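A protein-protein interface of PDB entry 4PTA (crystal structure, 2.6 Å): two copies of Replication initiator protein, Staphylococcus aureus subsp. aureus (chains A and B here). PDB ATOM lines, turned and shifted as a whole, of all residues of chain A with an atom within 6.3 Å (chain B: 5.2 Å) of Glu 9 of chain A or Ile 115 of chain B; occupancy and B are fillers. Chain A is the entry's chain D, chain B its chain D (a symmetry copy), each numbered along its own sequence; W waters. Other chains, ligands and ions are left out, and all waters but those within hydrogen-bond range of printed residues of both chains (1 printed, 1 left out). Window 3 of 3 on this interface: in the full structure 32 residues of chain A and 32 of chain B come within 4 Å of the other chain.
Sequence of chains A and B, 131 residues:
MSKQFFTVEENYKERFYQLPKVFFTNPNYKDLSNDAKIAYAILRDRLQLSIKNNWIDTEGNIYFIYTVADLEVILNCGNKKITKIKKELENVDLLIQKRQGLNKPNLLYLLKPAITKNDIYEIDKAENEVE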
ATOM      1  N   THR A   7       4.189  15.904 -27.666  1.00  0.00           N
ATOM      2  CA  THR A   7       3.167  16.908 -27.919  1.00  0.00           C
ATOM      3  C   THR A   7       1.916  16.653 -27.081  1.00  0.00           C
ATOM      4  O   THR A   7       1.590  15.507 -26.767  1.00  0.00           O
ATOM      5  CB  THR A   7       2.793  16.972 -29.413  1.00  0.00           C
ATOM      6  OG1 THR A   7       2.119  15.768 -29.795  1.00  0.00           O
ATOM      7  CG2 THR A   7       4.041  17.144 -30.267  1.00  0.00           C
ATOM      8  N   VAL A   8       1.225  17.729 -26.717  1.00  0.00           N
ATOM      9  CA  VAL A   8       0.011  17.628 -25.917  1.00  0.00           C
ATOM     10  C   VAL A   8      -1.066  16.863 -26.682  1.00  0.00           C
ATOM     11  O   VAL A   8      -1.931  16.220 -26.090  1.00  0.00           O
ATOM     12  CB  VAL A   8      -0.520  19.026 -25.522  1.00  0.00           C
ATOM     13  CG1 VAL A   8      -0.766  19.873 -26.756  1.00  0.00           C
ATOM     14  CG2 VAL A   8      -1.786  18.907 -24.686  1.00  0.00           C
ATOM     15  N   GLU A   9      -0.989  16.931 -28.007  1.00  0.00           N
ATOM     16  CA  GLU A   9      -1.950  16.277 -28.882  1.00  0.00           C
ATOM     17  C   GLU A   9      -1.733  14.766 -28.907  1.00  0.00           C
ATOM     18  O   GLU A   9      -2.679  13.990 -28.755  1.00  0.00           O
ATOM     19  CB  GLU A   9      -1.833  16.850 -30.292  1.00  0.00           C
ATOM     20  CG  GLU A   9      -2.907  16.396 -31.253  1.00  0.00           C
ATOM     21  CD  GLU A   9      -3.005  17.305 -32.461  1.00  0.00           C
ATOM     22  OE1 GLU A   9      -3.563  16.874 -33.489  1.00  0.00           O
ATOM     23  OE2 GLU A   9      -2.523  18.456 -32.379  1.00  0.00           O
ATOM     24  N   GLU A  10      -0.481  14.357 -29.100  1.00  0.00           N
ATOM     25  CA  GLU A  10      -0.123  12.947 -29.098  1.00  0.00           C
ATOM     26  C   GLU A  10      -0.403  12.359 -27.724  1.00  0.00           C
ATOM     27  O   GLU A  10      -0.730  11.181 -27.594  1.00  0.00           O
ATOM     28  CB  GLU A  10       1.356  12.773 -29.461  1.00  0.00           C
ATOM     29  CG  GLU A  10       1.861  11.339 -29.401  1.00  0.00           C
ATOM     30  CD  GLU A  10       1.249  10.456 -30.475  1.00  0.00           C
ATOM     31  OE1 GLU A  10       0.704  11.003 -31.461  1.00  0.00           O
ATOM     32  OE2 GLU A  10       1.311   9.215 -30.335  1.00  0.00           O
ATOM     33  N   ASN A  11      -0.280  13.197 -26.701  1.00  0.00           N
ATOM     34  CA  ASN A  11      -0.529  12.784 -25.327  1.00  0.00           C
ATOM     35  C   ASN A  11      -2.005  12.493 -25.055  1.00  0.00           C
ATOM     36  O   ASN A  11      -2.336  11.533 -24.362  1.00  0.00           O
ATOM     37  CB  ASN A  11      -0.009  13.842 -24.348  1.00  0.00           C
ATOM     38  CG  ASN A  11      -0.004  13.355 -22.911  1.00  0.00           C
ATOM     39  OD1 ASN A  11      -1.054  13.231 -22.282  1.00  0.00           O
ATOM     40  ND2 ASN A  11       1.182  13.086 -22.380  1.00  0.00           N
ATOM     41  N   TYR A  12      -2.890  13.324 -25.594  1.00  0.00           N
ATOM     42  CA  TYR A  12      -4.322  13.110 -25.412  1.00  0.00           C
ATOM     43  C   TYR A  12      -4.839  12.020 -26.341  1.00  0.00           C
ATOM     44  O   TYR A  12      -5.859  11.387 -26.073  1.00  0.00           O
ATOM     45  CB  TYR A  12      -5.101  14.418 -25.579  1.00  0.00           C
ATOM     46  CG  TYR A  12      -5.105  15.239 -24.312  1.00  0.00           C
ATOM     47  CD1 TYR A  12      -4.039  16.070 -23.996  1.00  0.00           C
ATOM     48  CD2 TYR A  12      -6.161  15.155 -23.414  1.00  0.00           C
ATOM     49  CE1 TYR A  12      -4.030  16.807 -22.829  1.00  0.00           C
ATOM     50  CE2 TYR A  12      -6.162  15.887 -22.243  1.00  0.00           C
ATOM     51  CZ  TYR A  12      -5.095  16.713 -21.955  1.00  0.00           C
ATOM     52  OH  TYR A  12      -5.096  17.445 -20.789  1.00  0.00           O
ATOM     53  N   LYS A  13      -4.104  11.793 -27.424  1.00  0.00           N
ATOM     54  CA  LYS A  13      -4.437  10.762 -28.395  1.00  0.00           C
ATOM     55  C   LYS A  13      -4.099   9.374 -27.851  1.00  0.00           C
ATOM     56  O   LYS A  13      -4.605   8.366 -28.343  1.00  0.00           O
ATOM     57  CB  LYS A  13      -3.675  11.024 -29.695  1.00  0.00           C
ATOM     58  CG  LYS A  13      -4.104  10.176 -30.877  1.00  0.00           C
ATOM     59  CD  LYS A  13      -3.394  10.628 -32.146  1.00  0.00           C
ATOM     60  CE  LYS A  13      -3.629  12.112 -32.400  1.00  0.00           C
ATOM     61  NZ  LYS A  13      -2.974  12.583 -33.647  1.00  0.00           N
ATOM     62  N   GLU A  14      -3.249   9.329 -26.829  1.00  0.00           N
ATOM     63  CA  GLU A  14      -2.828   8.067 -26.232  1.00  0.00           C
ATOM     64  C   GLU A  14      -3.505   7.806 -24.890  1.00  0.00           C
ATOM     65  O   GLU A  14      -2.972   7.077 -24.049  1.00  0.00           O
ATOM     66  CB  GLU A  14      -1.312   8.033 -26.048  1.00  0.00           C
ATOM     67  CG  GLU A  14      -0.516   8.002 -27.345  1.00  0.00           C
ATOM     68  CD  GLU A  14       0.983   8.052 -27.099  1.00  0.00           C
ATOM     69  OE1 GLU A  14       1.402   7.926 -25.926  1.00  0.00           O
ATOM     70  OE2 GLU A  14       1.743   8.223 -28.075  1.00  0.00           O
ATOM     71  N   VAL B  22     -11.112   9.801 -26.666  1.00  0.00           N
ATOM     72  CA  VAL B  22     -11.603  10.814 -27.590  1.00  0.00           C
ATOM     73  C   VAL B  22     -12.879  10.331 -28.280  1.00  0.00           C
ATOM     74  O   VAL B  22     -13.665  11.134 -28.776  1.00  0.00           O
ATOM     75  CB  VAL B  22     -10.535  11.235 -28.628  1.00  0.00           C
ATOM     76  CG1 VAL B  22     -10.122  10.051 -29.489  1.00  0.00           C
ATOM     77  CG2 VAL B  22     -11.057  12.367 -29.489  1.00  0.00           C
ATOM     78  N   PRO B 113      -7.031   8.237 -34.027  1.00  0.00           N
ATOM     79  CA  PRO B 113      -8.029   9.307 -34.043  1.00  0.00           C
ATOM     80  C   PRO B 113      -7.404  10.695 -34.090  1.00  0.00           C
ATOM     81  O   PRO B 113      -6.199  10.855 -33.891  1.00  0.00           O
ATOM     82  CB  PRO B 113      -8.759   9.116 -32.715  1.00  0.00           C
ATOM     83  CG  PRO B 113      -7.750   8.463 -31.826  1.00  0.00           C
ATOM     84  CD  PRO B 113      -6.935   7.577 -32.710  1.00  0.00           C
ATOM     85  N   ALA B 114      -8.234  11.695 -34.355  1.00  0.00           N
ATOM     86  CA  ALA B 114      -7.790  13.075 -34.315  1.00  0.00           C
ATOM     87  C   ALA B 114      -8.022  13.659 -32.928  1.00  0.00           C
ATOM     88  O   ALA B 114      -8.818  13.140 -32.145  1.00  0.00           O
ATOM     89  CB  ALA B 114      -8.513  13.893 -35.371  1.00  0.00           C
ATOM     90  N   ILE B 115      -7.314  14.738 -32.626  1.00  0.00           N
ATOM     91  CA  ILE B 115      -7.477  15.432 -31.360  1.00  0.00           C
ATOM     92  C   ILE B 115      -7.559  16.922 -31.635  1.00  0.00           C
ATOM     93  O   ILE B 115      -6.840  17.440 -32.489  1.00  0.00           O
ATOM     94  CB  ILE B 115      -6.302  15.148 -30.408  1.00  0.00           C
ATOM     95  CG1 ILE B 115      -6.299  13.678 -29.989  1.00  0.00           C
ATOM     96  CG2 ILE B 115      -6.379  16.041 -29.176  1.00  0.00           C
ATOM     97  CD1 ILE B 115      -7.376  13.328 -28.986  1.00  0.00           C
ATOM     98  N   THR B 116      -8.452  17.602 -30.924  1.00  0.00           N
ATOM     99  CA  THR B 116      -8.601  19.045 -31.056  1.00  0.00           C
ATOM    100  C   THR B 116      -8.450  19.694 -29.694  1.00  0.00           C
ATOM    101  O   THR B 116      -8.577  19.028 -28.668  1.00  0.00           O
ATOM    102  CB  THR B 116      -9.979  19.428 -31.610  1.00  0.00           C
ATOM    103  OG1 THR B 116     -10.992  19.112 -30.643  1.00  0.00           O
ATOM    104  CG2 THR B 116     -10.258  18.695 -32.922  1.00  0.00           C
ATOM    105  N   LYS B 117      -8.180  20.996 -29.690  1.00  0.00           N
ATOM    106  CA  LYS B 117      -8.075  21.745 -28.444  1.00  0.00           C
ATOM    107  C   LYS B 117      -9.295  21.509 -27.556  1.00  0.00           C
ATOM    108  O   LYS B 117      -9.190  21.512 -26.331  1.00  0.00           O
ATOM    109  CB  LYS B 117      -7.912  23.241 -28.722  1.00  0.00           C
ATOM    110  CG  LYS B 117      -6.616  23.619 -29.423  1.00  0.00           C
ATOM    111  CD  LYS B 117      -6.474  25.134 -29.510  1.00  0.00           C
ATOM    112  CE  LYS B 117      -5.210  25.543 -30.252  1.00  0.00           C
ATOM    113  NZ  LYS B 117      -5.042  27.025 -30.269  1.00  0.00           N
ATOM    114  N   ASP B 119     -11.239  18.660 -27.609  1.00  0.00           N
ATOM    115  CA  ASP B 119     -11.077  17.303 -27.104  1.00  0.00           C
ATOM    116  C   ASP B 119     -10.230  17.329 -25.839  1.00  0.00           C
ATOM    117  O   ASP B 119     -10.607  16.765 -24.813  1.00  0.00           O
ATOM    118  CB  ASP B 119     -10.426  16.404 -28.154  1.00  0.00           C
ATOM    119  CG  ASP B 119     -11.356  16.084 -29.304  1.00  0.00           C
ATOM    120  OD1 ASP B 119     -12.553  15.843 -29.044  1.00  0.00           O
ATOM    121  OD2 ASP B 119     -10.895  16.072 -30.466  1.00  0.00           O
ATOM    122  N   ILE B 120      -9.083  17.993 -25.922  1.00  0.00           N
ATOM    123  CA  ILE B 120      -8.213  18.163 -24.770  1.00  0.00           C
ATOM    124  C   ILE B 120      -8.992  18.733 -23.581  1.00  0.00           C
ATOM    125  O   ILE B 120      -9.039  18.122 -22.512  1.00  0.00           O
ATOM    126  CB  ILE B 120      -7.006  19.057 -25.116  1.00  0.00           C
ATOM    127  CG1 ILE B 120      -6.125  18.360 -26.157  1.00  0.00           C
ATOM    128  CG2 ILE B 120      -6.209  19.400 -23.862  1.00  0.00           C
ATOM    129  CD1 ILE B 120      -5.071  19.254 -26.786  1.00  0.00           C
ATOM    130  N   ILE B 123     -11.527  16.213 -22.446  1.00  0.00           N
ATOM    131  CA  ILE B 123     -10.859  15.069 -21.833  1.00  0.00           C
ATOM    132  C   ILE B 123     -10.358  15.397 -20.426  1.00  0.00           C
ATOM    133  O   ILE B 123     -10.321  14.529 -19.556  1.00  0.00           O
ATOM    134  CB  ILE B 123      -9.706  14.534 -22.711  1.00  0.00           C
ATOM    135  CG1 ILE B 123     -10.260  13.915 -23.998  1.00  0.00           C
ATOM    136  CG2 ILE B 123      -8.891  13.497 -21.955  1.00  0.00           C
ATOM    137  CD1 ILE B 123      -9.193  13.420 -24.951  1.00  0.00           C
HETATM  138  O   HOH W   1      -7.813   9.963 -26.751  1.00  0.00           O
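Glu 9 of chain A touches one residue of chain B. Ile 115 of chain B touches just these residues of chain A: Glu 9 (3.5 Å), Tyr 12 (3.8 Å) and Lys 13 (3.7 Å). Printed residues of chain A within 4 Å of Ile 120 of chain B: Val 8 and Tyr 12. Printed residues of chain B within 4 Å of Lys 13 of chain A: Pro 113 and Ile 115. Printed residues of chain B within 4 Å of Tyr 12 of chain A: Ile 115, Ile 120 and Ile 123. Printed residues of chain A within 4 Å of Pro 113 of chain B: Lys 13. Asp 119 of chain B touches none of the printed residues of chain A. Ala 114 of chain B touches none of the printed residues of chain A. The nearest residue of chain B that does not touch Glu 9 of chain A is Ile 120 of chain B (4.8 Å). The nearest residue of chain A that does not touch Ile 115 of chain B is Val 8 of chain A (5.4 Å).
Val 8 of chain A touches Ile 120 of chain B. O of Tyr 12 of chain A touches CD1 of Ile 115 of chain B, 3.8 Å away. Ile 120 of chain B touches Tyr 12 of chain A (CG2 to CZ, 3.5 Å). Ile 123 of chain B touches Tyr 12 of chain A (CG2 to CD2, 3.5 Å). Pro 113 of chain B touches Lys 13 of chain A. Lys 13 of chain A touches Ile 115 of chain B.
Water W1 bridges the backbone carbonyl oxygen (O) of Tyr 12 of chain A and the backbone NH (N) of Val 22 of chain B.
Printed residues of chain A that touch a printed residue of chain B: Val 8, Glu 9, Tyr 12 and Lys 13. Among the printed residues, 7 pairs touch across the chains. Among the printed residues, no Asp or Glu carboxylate lies within 4 Å of a Lys or Arg side-chain nitrogen of the other chain.
No position is printed for both chains. Of the 7 pairs that touch across the chains among the printed residues, none has its exchanged pair printed and touching as well.
OE1 of Glu 9 of chain A lies close to O of Ile 115 of chain B (3.5 Å).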
